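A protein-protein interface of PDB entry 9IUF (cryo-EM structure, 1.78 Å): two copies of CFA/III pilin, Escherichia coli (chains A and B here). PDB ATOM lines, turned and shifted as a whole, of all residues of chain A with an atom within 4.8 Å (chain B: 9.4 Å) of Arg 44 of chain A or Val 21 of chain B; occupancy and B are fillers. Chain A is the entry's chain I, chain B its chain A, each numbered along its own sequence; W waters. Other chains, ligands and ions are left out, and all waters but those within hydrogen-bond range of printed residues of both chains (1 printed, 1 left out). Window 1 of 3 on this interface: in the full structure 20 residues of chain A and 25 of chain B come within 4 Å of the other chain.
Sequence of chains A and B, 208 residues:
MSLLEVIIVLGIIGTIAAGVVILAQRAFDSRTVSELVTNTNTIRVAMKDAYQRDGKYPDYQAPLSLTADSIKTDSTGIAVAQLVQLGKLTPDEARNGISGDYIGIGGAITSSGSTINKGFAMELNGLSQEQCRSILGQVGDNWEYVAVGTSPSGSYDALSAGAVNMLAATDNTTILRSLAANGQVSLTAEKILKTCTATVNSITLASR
ND2 of Asn 142 of chain A is in hydrogen-bond range of O of Ala 18 of chain B. The guanidinium group of Arg 44 of chain A lies close to the side-chain amide nitrogen of Gln 25 of chain B, at 3.0 Å.
The side-chain carboxylate (OD1) of Asp 29 of chain B sits close to the side-chain amide oxygen (OE1) of Gln 25 of chain B (2.8 Å). The guanidinium group (NH1) of Arg 44 of chain A sits at hydrogen-bond distance from the backbone carbonyl oxygen (O) of Asn 142 of chain A (3.3 Å). NE of Arg 44 of chain A sits at hydrogen-bond distance from OG of Ser 207 of chain A.
Among the printed residues, merely in contact across the chains: Asn 41 of chain A with Val 20 of chain B (3.8 Å), Asn 41 of chain A with Val 21 of chain B (3.5 Å), Arg 44 of chain A with Val 21 of chain B (3.8 Å), Lys 48 of chain A with Phe 28 of chain B (3.0 Å), Asn 142 of chain A with Val 21 of chain B (3.9 Å) and Asn 142 of chain A with Ile 22 of chain B (3.4 Å).
Arg 44 of chain A touches just these residues of chain B: Val 21 (3.8 Å) and Gln 25 (3.0 Å). Val 21 of chain B touches just these residues of chain A: Asn 41 (3.5 Å), Arg 44 (3.8 Å) and Asn 142 (3.9 Å). Of chain B, only Val 20 (3.8 Å) and Val 21 (3.5 Å) come within 4 Å of Asn 41 of chain A. No residue of chain B comes within 4 Å of Val 45 of chain A. Printed residues of chain B within 4 Å of Lys 48 of chain A: Phe 28 (3.0 Å). Printed residues of chain A within 4 Å of Ala 18 of chain B: Asn 142 (2.9 Å). Of the printed residues of chain B, Asn 142 of chain A touches Ala 18, Val 21 and Ile 22. Phe 120 of chain A touches none of the printed residues of chain B. The nearest residue of chain B that does not touch Arg 44 of chain A is Ile 22 of chain B (6.4 Å).
Of the 16 printed residues of chain A, 4 touch a printed residue of chain B. Of the 18 printed residues of chain B, 6 touch a printed residue of chain A. Among the printed residues, 8 pairs touch across the chains. Among the printed residues, no Asp or Glu carboxylate lies within 4 Å of a Lys or Arg side-chain nitrogen of the other chain.
No position is printed for both chains. Of the 8 pairs that touch across the chains among the printed residues, none has its exchanged pair printed and touching as well.
Water W1 bridges ND2 of Asn 41 of chain A (2.8 Å) and O of Val 21 of chain B (3.0 Å).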
ATOM      1  N   VAL A  37       3.547 -33.824  21.829  1.00  0.00           N
ATOM      2  CA  VAL A  37       4.734 -33.083  22.253  1.00  0.00           C
ATOM      3  C   VAL A  37       5.261 -32.228  21.104  1.00  0.00           C
ATOM      4  O   VAL A  37       5.497 -31.016  21.253  1.00  0.00           O
ATOM      5  CB  VAL A  37       5.810 -34.050  22.777  1.00  0.00           C
ATOM      6  CG1 VAL A  37       7.134 -33.329  22.962  1.00  0.00           C
ATOM      7  CG2 VAL A  37       5.360 -34.692  24.081  1.00  0.00           C
ATOM      8  N   THR A  40       2.742 -29.348  20.209  1.00  0.00           N
ATOM      9  CA  THR A  40       2.732 -28.288  21.208  1.00  0.00           C
ATOM     10  C   THR A  40       3.973 -27.418  21.088  1.00  0.00           C
ATOM     11  O   THR A  40       3.891 -26.192  21.219  1.00  0.00           O
ATOM     12  CB  THR A  40       2.619 -28.872  22.616  1.00  0.00           C
ATOM     13  OG1 THR A  40       3.549 -29.951  22.768  1.00  0.00           O
ATOM     14  CG2 THR A  40       1.208 -29.375  22.870  1.00  0.00           C
ATOM     15  N   ASN A  41       5.135 -28.027  20.827  1.00  0.00           N
ATOM     16  CA  ASN A  41       6.326 -27.211  20.598  1.00  0.00           C
ATOM     17  C   ASN A  41       6.168 -26.333  19.360  1.00  0.00           C
ATOM     18  O   ASN A  41       6.539 -25.150  19.373  1.00  0.00           O
ATOM     19  CB  ASN A  41       7.560 -28.093  20.459  1.00  0.00           C
ATOM     20  CG  ASN A  41       8.835 -27.286  20.349  1.00  0.00           C
ATOM     21  OD1 ASN A  41       9.683 -27.552  19.499  1.00  0.00           O
ATOM     22  ND2 ASN A  41       8.974 -26.284  21.207  1.00  0.00           N
ATOM     23  N   THR A  42       5.633 -26.902  18.278  1.00  0.00           N
ATOM     24  CA  THR A  42       5.429 -26.124  17.059  1.00  0.00           C
ATOM     25  C   THR A  42       4.476 -24.962  17.306  1.00  0.00           C
ATOM     26  O   THR A  42       4.715 -23.841  16.842  1.00  0.00           O
ATOM     27  CB  THR A  42       4.897 -27.023  15.943  1.00  0.00           C
ATOM     28  OG1 THR A  42       5.794 -28.122  15.744  1.00  0.00           O
ATOM     29  CG2 THR A  42       4.768 -26.244  14.647  1.00  0.00           C
ATOM     30  N   ILE A  43       3.396 -25.212  18.047  1.00  0.00           N
ATOM     31  CA  ILE A  43       2.438 -24.162  18.374  1.00  0.00           C
ATOM     32  C   ILE A  43       3.095 -23.086  19.225  1.00  0.00           C
ATOM     33  O   ILE A  43       2.846 -21.895  19.037  1.00  0.00           O
ATOM     34  CB  ILE A  43       1.206 -24.764  19.075  1.00  0.00           C
ATOM     35  CG1 ILE A  43       0.356 -25.546  18.077  1.00  0.00           C
ATOM     36  CG2 ILE A  43       0.380 -23.679  19.740  1.00  0.00           C
ATOM     37  CD1 ILE A  43      -0.824 -26.240  18.702  1.00  0.00           C
ATOM     38  N   ARG A  44       3.930 -23.489  20.183  1.00  0.00           N
ATOM     39  CA  ARG A  44       4.609 -22.517  21.034  1.00  0.00           C
ATOM     40  C   ARG A  44       5.501 -21.596  20.208  1.00  0.00           C
ATOM     41  O   ARG A  44       5.448 -20.366  20.345  1.00  0.00           O
ATOM     42  CB  ARG A  44       5.419 -23.258  22.098  1.00  0.00           C
ATOM     43  CG  ARG A  44       6.302 -22.392  22.974  1.00  0.00           C
ATOM     44  CD  ARG A  44       7.191 -23.276  23.833  1.00  0.00           C
ATOM     45  NE  ARG A  44       7.852 -22.544  24.905  1.00  0.00           N
ATOM     46  CZ  ARG A  44       8.460 -23.116  25.934  1.00  0.00           C
ATOM     47  NH1 ARG A  44       8.514 -24.432  26.058  1.00  0.00           N
ATOM     48  NH2 ARG A  44       9.024 -22.352  26.863  1.00  0.00           N
ATOM     49  N   VAL A  45       6.311 -22.181  19.323  1.00  0.00           N
ATOM     50  CA  VAL A  45       7.196 -21.374  18.483  1.00  0.00           C
ATOM     51  C   VAL A  45       6.385 -20.462  17.569  1.00  0.00           C
ATOM     52  O   VAL A  45       6.691 -19.270  17.421  1.00  0.00           O
ATOM     53  CB  VAL A  45       8.146 -22.284  17.682  1.00  0.00           C
ATOM     54  CG1 VAL A  45       8.998 -21.460  16.733  1.00  0.00           C
ATOM     55  CG2 VAL A  45       9.022 -23.093  18.623  1.00  0.00           C
ATOM     56  N   ALA A  46       5.333 -21.005  16.947  1.00  0.00           N
ATOM     57  CA  ALA A  46       4.515 -20.215  16.035  1.00  0.00           C
ATOM     58  C   ALA A  46       3.814 -19.074  16.758  1.00  0.00           C
ATOM     59  O   ALA A  46       3.717 -17.963  16.227  1.00  0.00           O
ATOM     60  CB  ALA A  46       3.494 -21.114  15.340  1.00  0.00           C
ATOM     61  N   MET A  47       3.300 -19.332  17.961  1.00  0.00           N
ATOM     62  CA  MET A  47       2.629 -18.289  18.726  1.00  0.00           C
ATOM     63  C   MET A  47       3.607 -17.196  19.118  1.00  0.00           C
ATOM     64  O   MET A  47       3.275 -16.006  19.067  1.00  0.00           O
ATOM     65  CB  MET A  47       1.976 -18.886  19.973  1.00  0.00           C
ATOM     66  CG  MET A  47       0.624 -19.531  19.725  1.00  0.00           C
ATOM     67  SD  MET A  47      -0.758 -18.380  19.727  1.00  0.00           S
ATOM     68  CE  MET A  47      -0.544 -17.582  21.311  1.00  0.00           C
ATOM     69  N   LYS A  48       4.821 -17.581  19.516  1.00  0.00           N
ATOM     70  CA  LYS A  48       5.814 -16.582  19.890  1.00  0.00           C
ATOM     71  C   LYS A  48       6.201 -15.723  18.693  1.00  0.00           C
ATOM     72  O   LYS A  48       6.391 -14.508  18.826  1.00  0.00           O
ATOM     73  CB  LYS A  48       7.038 -17.267  20.490  1.00  0.00           C
ATOM     74  CG  LYS A  48       6.978 -17.385  22.001  1.00  0.00           C
ATOM     75  CD  LYS A  48       7.891 -18.488  22.499  1.00  0.00           C
ATOM     76  CE  LYS A  48       9.270 -17.956  22.819  1.00  0.00           C
ATOM     77  NZ  LYS A  48       9.204 -16.960  23.921  1.00  0.00           N
ATOM     78  N   PHE A 120       1.035 -17.125  26.857  1.00  0.00           N
ATOM     79  CA  PHE A 120      -0.027 -17.926  26.271  1.00  0.00           C
ATOM     80  C   PHE A 120      -0.015 -19.325  26.863  1.00  0.00           C
ATOM     81  O   PHE A 120       1.037 -19.864  27.214  1.00  0.00           O
ATOM     82  CB  PHE A 120       0.091 -17.998  24.743  1.00  0.00           C
ATOM     83  CG  PHE A 120       1.379 -18.593  24.258  1.00  0.00           C
ATOM     84  CD1 PHE A 120       2.489 -17.794  24.052  1.00  0.00           C
ATOM     85  CD2 PHE A 120       1.477 -19.948  24.000  1.00  0.00           C
ATOM     86  CE1 PHE A 120       3.674 -18.337  23.604  1.00  0.00           C
ATOM     87  CE2 PHE A 120       2.661 -20.496  23.553  1.00  0.00           C
ATOM     88  CZ  PHE A 120       3.760 -19.689  23.355  1.00  0.00           C
ATOM     89  N   MET A 122      -1.878 -23.374  26.401  1.00  0.00           N
ATOM     90  CA  MET A 122      -2.611 -24.313  25.569  1.00  0.00           C
ATOM     91  C   MET A 122      -3.051 -25.492  26.422  1.00  0.00           C
ATOM     92  O   MET A 122      -2.366 -25.890  27.368  1.00  0.00           O
ATOM     93  CB  MET A 122      -1.777 -24.796  24.374  1.00  0.00           C
ATOM     94  CG  MET A 122      -0.553 -25.609  24.741  1.00  0.00           C
ATOM     95  SD  MET A 122       0.629 -25.688  23.383  1.00  0.00           S
ATOM     96  CE  MET A 122       1.194 -23.991  23.331  1.00  0.00           C
ATOM     97  N   VAL A 139       7.770 -34.294  28.617  1.00  0.00           N
ATOM     98  CA  VAL A 139       7.962 -32.893  28.260  1.00  0.00           C
ATOM     99  C   VAL A 139       7.666 -31.914  29.389  1.00  0.00           C
ATOM    100  O   VAL A 139       7.837 -30.708  29.198  1.00  0.00           O
ATOM    101  CB  VAL A 139       7.131 -32.533  27.009  1.00  0.00           C
ATOM    102  CG1 VAL A 139       5.722 -32.093  27.391  1.00  0.00           C
ATOM    103  CG2 VAL A 139       7.840 -31.473  26.173  1.00  0.00           C
ATOM    104  N   ASN A 142      10.179 -29.210  30.468  1.00  0.00           N
ATOM    105  CA  ASN A 142      10.581 -28.274  29.429  1.00  0.00           C
ATOM    106  C   ASN A 142       9.644 -27.080  29.302  1.00  0.00           C
ATOM    107  O   ASN A 142       9.902 -26.197  28.478  1.00  0.00           O
ATOM    108  CB  ASN A 142      10.678 -28.999  28.085  1.00  0.00           C
ATOM    109  CG  ASN A 142      11.676 -30.137  28.109  1.00  0.00           C
ATOM    110  OD1 ASN A 142      12.376 -30.342  29.100  1.00  0.00           O
ATOM    111  ND2 ASN A 142      11.748 -30.885  27.016  1.00  0.00           N
ATOM    112  N   TRP A 143       8.574 -27.025  30.088  1.00  0.00           N
ATOM    113  CA  TRP A 143       7.631 -25.919  30.055  1.00  0.00           C
ATOM    114  C   TRP A 143       7.653 -25.185  31.388  1.00  0.00           C
ATOM    115  O   TRP A 143       7.838 -25.792  32.446  1.00  0.00           O
ATOM    116  CB  TRP A 143       6.210 -26.403  29.750  1.00  0.00           C
ATOM    117  CG  TRP A 143       6.016 -26.826  28.330  1.00  0.00           C
ATOM    118  CD1 TRP A 143       6.453 -27.981  27.753  1.00  0.00           C
ATOM    119  CD2 TRP A 143       5.338 -26.097  27.302  1.00  0.00           C
ATOM    120  NE1 TRP A 143       6.087 -28.018  26.431  1.00  0.00           N
ATOM    121  CE2 TRP A 143       5.401 -26.872  26.130  1.00  0.00           C
ATOM    122  CE3 TRP A 143       4.681 -24.863  27.261  1.00  0.00           C
ATOM    123  CZ2 TRP A 143       4.833 -26.456  24.929  1.00  0.00           C
ATOM    124  CZ3 TRP A 143       4.118 -24.453  26.070  1.00  0.00           C
ATOM    125  CH2 TRP A 143       4.197 -25.247  24.920  1.00  0.00           C
ATOM    126  N   SER A 207       3.454 -20.710  28.602  1.00  0.00           N
ATOM    127  CA  SER A 207       4.766 -20.138  28.356  1.00  0.00           C
ATOM    128  C   SER A 207       4.621 -18.631  28.215  1.00  0.00           C
ATOM    129  O   SER A 207       3.523 -18.108  28.011  1.00  0.00           O
ATOM    130  CB  SER A 207       5.409 -20.734  27.097  1.00  0.00           C
ATOM    131  OG  SER A 207       6.362 -19.847  26.539  1.00  0.00           O
ATOM    132  N   ILE B  13      11.645 -41.189  19.674  1.00  0.00           N
ATOM    133  CA  ILE B  13      11.239 -40.016  18.903  1.00  0.00           C
ATOM    134  C   ILE B  13      10.703 -38.928  19.826  1.00  0.00           C
ATOM    135  O   ILE B  13      11.015 -37.740  19.660  1.00  0.00           O
ATOM    136  CB  ILE B  13      10.205 -40.417  17.835  1.00  0.00           C
ATOM    137  CG1 ILE B  13      10.873 -41.232  16.727  1.00  0.00           C
ATOM    138  CG2 ILE B  13       9.520 -39.191  17.254  1.00  0.00           C
ATOM    139  CD1 ILE B  13       9.899 -41.831  15.740  1.00  0.00           C
ATOM    140  N   GLY B  14       9.888 -39.311  20.809  1.00  0.00           N
ATOM    141  CA  GLY B  14       9.378 -38.334  21.760  1.00  0.00           C
ATOM    142  C   GLY B  14      10.477 -37.688  22.582  1.00  0.00           C
ATOM    143  O   GLY B  14      10.434 -36.485  22.866  1.00  0.00           O
ATOM    144  N   THR B  15      11.476 -38.479  22.987  1.00  0.00           N
ATOM    145  CA  THR B  15      12.613 -37.911  23.708  1.00  0.00           C
ATOM    146  C   THR B  15      13.342 -36.876  22.857  1.00  0.00           C
ATOM    147  O   THR B  15      13.693 -35.786  23.338  1.00  0.00           O
ATOM    148  CB  THR B  15      13.569 -39.027  24.134  1.00  0.00           C
ATOM    149  OG1 THR B  15      12.898 -39.912  25.038  1.00  0.00           O
ATOM    150  CG2 THR B  15      14.796 -38.450  24.820  1.00  0.00           C
ATOM    151  N   ILE B  16      13.564 -37.194  21.579  1.00  0.00           N
ATOM    152  CA  ILE B  16      14.219 -36.245  20.681  1.00  0.00           C
ATOM    153  C   ILE B  16      13.379 -34.980  20.534  1.00  0.00           C
ATOM    154  O   ILE B  16      13.909 -33.862  20.495  1.00  0.00           O
ATOM    155  CB  ILE B  16      14.500 -36.909  19.319  1.00  0.00           C
ATOM    156  CG1 ILE B  16      15.561 -37.999  19.474  1.00  0.00           C
ATOM    157  CG2 ILE B  16      14.948 -35.879  18.298  1.00  0.00           C
ATOM    158  CD1 ILE B  16      15.678 -38.911  18.276  1.00  0.00           C
ATOM    159  N   ALA B  17      12.054 -35.134  20.462  1.00  0.00           N
ATOM    160  CA  ALA B  17      11.177 -33.971  20.348  1.00  0.00           C
ATOM    161  C   ALA B  17      11.273 -33.071  21.579  1.00  0.00           C
ATOM    162  O   ALA B  17      11.287 -31.839  21.459  1.00  0.00           O
ATOM    163  CB  ALA B  17       9.736 -34.424  20.123  1.00  0.00           C
ATOM    164  N   ALA B  18      11.327 -33.667  22.772  1.00  0.00           N
ATOM    165  CA  ALA B  18      11.483 -32.863  23.983  1.00  0.00           C
ATOM    166  C   ALA B  18      12.811 -32.110  23.979  1.00  0.00           C
ATOM    167  O   ALA B  18      12.880 -30.927  24.366  1.00  0.00           O
ATOM    168  CB  ALA B  18      11.371 -33.754  25.220  1.00  0.00           C
ATOM    169  N   GLY B  19      13.881 -32.780  23.545  1.00  0.00           N
ATOM    170  CA  GLY B  19      15.148 -32.084  23.386  1.00  0.00           C
ATOM    171  C   GLY B  19      15.040 -30.906  22.435  1.00  0.00           C
ATOM    172  O   GLY B  19      15.630 -29.845  22.668  1.00  0.00           O
ATOM    173  N   VAL B  20      14.279 -31.078  21.352  1.00  0.00           N
ATOM    174  CA  VAL B  20      14.064 -29.984  20.407  1.00  0.00           C
ATOM    175  C   VAL B  20      13.330 -28.833  21.081  1.00  0.00           C
ATOM    176  O   VAL B  20      13.604 -27.659  20.808  1.00  0.00           O
ATOM    177  CB  VAL B  20      13.309 -30.493  19.165  1.00  0.00           C
ATOM    178  CG1 VAL B  20      12.846 -29.327  18.305  1.00  0.00           C
ATOM    179  CG2 VAL B  20      14.192 -31.426  18.360  1.00  0.00           C
ATOM    180  N   VAL B  21      12.378 -29.148  21.962  1.00  0.00           N
ATOM    181  CA  VAL B  21      11.681 -28.100  22.708  1.00  0.00           C
ATOM    182  C   VAL B  21      12.683 -27.253  23.484  1.00  0.00           C
ATOM    183  O   VAL B  21      12.684 -26.012  23.409  1.00  0.00           O
ATOM    184  CB  VAL B  21      10.635 -28.714  23.657  1.00  0.00           C
ATOM    185  CG1 VAL B  21       9.959 -27.628  24.481  1.00  0.00           C
ATOM    186  CG2 VAL B  21       9.618 -29.533  22.892  1.00  0.00           C
ATOM    187  N   ILE B  22      13.562 -27.924  24.233  1.00  0.00           N
ATOM    188  CA  ILE B  22      14.544 -27.203  25.045  1.00  0.00           C
ATOM    189  C   ILE B  22      15.451 -26.352  24.158  1.00  0.00           C
ATOM    190  O   ILE B  22      15.724 -25.177  24.453  1.00  0.00           O
ATOM    191  CB  ILE B  22      15.359 -28.186  25.904  1.00  0.00           C
ATOM    192  CG1 ILE B  22      14.561 -28.603  27.137  1.00  0.00           C
ATOM    193  CG2 ILE B  22      16.680 -27.565  26.325  1.00  0.00           C
ATOM    194  CD1 ILE B  22      14.131 -27.444  28.004  1.00  0.00           C
ATOM    195  N   LEU B  23      15.928 -26.935  23.056  1.00  0.00           N
ATOM    196  CA  LEU B  23      16.855 -26.221  22.184  1.00  0.00           C
ATOM    197  C   LEU B  23      16.198 -25.004  21.543  1.00  0.00           C
ATOM    198  O   LEU B  23      16.830 -23.951  21.412  1.00  0.00           O
ATOM    199  CB  LEU B  23      17.401 -27.163  21.114  1.00  0.00           C
ATOM    200  CG  LEU B  23      18.448 -28.166  21.597  1.00  0.00           C
ATOM    201  CD1 LEU B  23      19.113 -28.853  20.418  1.00  0.00           C
ATOM    202  CD2 LEU B  23      19.482 -27.479  22.473  1.00  0.00           C
ATOM    203  N   ALA B  24      14.937 -25.131  21.123  1.00  0.00           N
ATOM    204  CA  ALA B  24      14.240 -23.997  20.529  1.00  0.00           C
ATOM    205  C   ALA B  24      14.072 -22.870  21.536  1.00  0.00           C
ATOM    206  O   ALA B  24      14.253 -21.691  21.198  1.00  0.00           O
ATOM    207  CB  ALA B  24      12.884 -24.438  19.982  1.00  0.00           C
ATOM    208  N   GLN B  25      13.731 -23.211  22.782  1.00  0.00           N
ATOM    209  CA  GLN B  25      13.623 -22.171  23.802  1.00  0.00           C
ATOM    210  C   GLN B  25      14.958 -21.460  24.007  1.00  0.00           C
ATOM    211  O   GLN B  25      15.010 -20.223  24.082  1.00  0.00           O
ATOM    212  CB  GLN B  25      13.122 -22.769  25.116  1.00  0.00           C
ATOM    213  CG  GLN B  25      12.955 -21.754  26.236  1.00  0.00           C
ATOM    214  CD  GLN B  25      12.121 -20.557  25.825  1.00  0.00           C
ATOM    215  OE1 GLN B  25      12.504 -19.412  26.059  1.00  0.00           O
ATOM    216  NE2 GLN B  25      10.973 -20.814  25.212  1.00  0.00           N
ATOM    217  N   ARG B  26      16.051 -22.225  24.085  1.00  0.00           N
ATOM    218  CA  ARG B  26      17.360 -21.606  24.281  1.00  0.00           C
ATOM    219  C   ARG B  26      17.743 -20.719  23.100  1.00  0.00           C
ATOM    220  O   ARG B  26      18.322 -19.642  23.285  1.00  0.00           O
ATOM    221  CB  ARG B  26      18.426 -22.674  24.514  1.00  0.00           C
ATOM    222  CG  ARG B  26      19.812 -22.101  24.763  1.00  0.00           C
ATOM    223  CD  ARG B  26      20.776 -23.155  25.273  1.00  0.00           C
ATOM    224  NE  ARG B  26      20.230 -23.889  26.406  1.00  0.00           N
ATOM    225  CZ  ARG B  26      20.395 -25.189  26.602  1.00  0.00           C
ATOM    226  NH1 ARG B  26      21.090 -25.933  25.759  1.00  0.00           N
ATOM    227  NH2 ARG B  26      19.849 -25.757  27.673  1.00  0.00           N
ATOM    228  N   ALA B  27      17.440 -21.162  21.878  1.00  0.00           N
ATOM    229  CA  ALA B  27      17.761 -20.361  20.699  1.00  0.00           C
ATOM    230  C   ALA B  27      16.982 -19.053  20.694  1.00  0.00           C
ATOM    231  O   ALA B  27      17.534 -17.992  20.370  1.00  0.00           O
ATOM    232  CB  ALA B  27      17.479 -21.160  19.429  1.00  0.00           C
ATOM    233  N   PHE B  28      15.694 -19.107  21.047  1.00  0.00           N
ATOM    234  CA  PHE B  28      14.915 -17.878  21.141  1.00  0.00           C
ATOM    235  C   PHE B  28      15.509 -16.936  22.179  1.00  0.00           C
ATOM    236  O   PHE B  28      15.623 -15.726  21.939  1.00  0.00           O
ATOM    237  CB  PHE B  28      13.458 -18.195  21.480  1.00  0.00           C
ATOM    238  CG  PHE B  28      12.619 -16.975  21.749  1.00  0.00           C
ATOM    239  CD1 PHE B  28      12.007 -16.299  20.709  1.00  0.00           C
ATOM    240  CD2 PHE B  28      12.445 -16.503  23.040  1.00  0.00           C
ATOM    241  CE1 PHE B  28      11.237 -15.177  20.949  1.00  0.00           C
ATOM    242  CE2 PHE B  28      11.681 -15.379  23.285  1.00  0.00           C
ATOM    243  CZ  PHE B  28      11.073 -14.718  22.238  1.00  0.00           C
ATOM    244  N   ASP B  29      15.898 -17.476  23.338  1.00  0.00           N
ATOM    245  CA  ASP B  29      16.493 -16.636  24.374  1.00  0.00           C
ATOM    246  C   ASP B  29      17.779 -15.980  23.888  1.00  0.00           C
ATOM    247  O   ASP B  29      17.999 -14.786  24.119  1.00  0.00           O
ATOM    248  CB  ASP B  29      16.756 -17.460  25.633  1.00  0.00           C
ATOM    249  CG  ASP B  29      15.494 -17.735  26.419  1.00  0.00           C
ATOM    250  OD1 ASP B  29      14.401 -17.400  25.920  1.00  0.00           O
ATOM    251  OD2 ASP B  29      15.594 -18.287  27.535  1.00  0.00           O
ATOM    252  N   GLN B 131      17.545 -15.220  31.104  1.00  0.00           N
ATOM    253  CA  GLN B 131      17.745 -14.046  30.260  1.00  0.00           C
ATOM    254  C   GLN B 131      18.418 -12.917  31.030  1.00  0.00           C
ATOM    255  O   GLN B 131      19.302 -12.238  30.494  1.00  0.00           O
ATOM    256  CB  GLN B 131      16.409 -13.580  29.684  1.00  0.00           C
ATOM    257  CG  GLN B 131      15.832 -14.508  28.632  1.00  0.00           C
ATOM    258  CD  GLN B 131      14.320 -14.472  28.593  1.00  0.00           C
ATOM    259  OE1 GLN B 131      13.682 -13.816  29.414  1.00  0.00           O
ATOM    260  NE2 GLN B 131      13.736 -15.181  27.635  1.00  0.00           N
HETATM  261  O   HOH W   1      10.304 -24.326  22.619  1.00  0.00           O
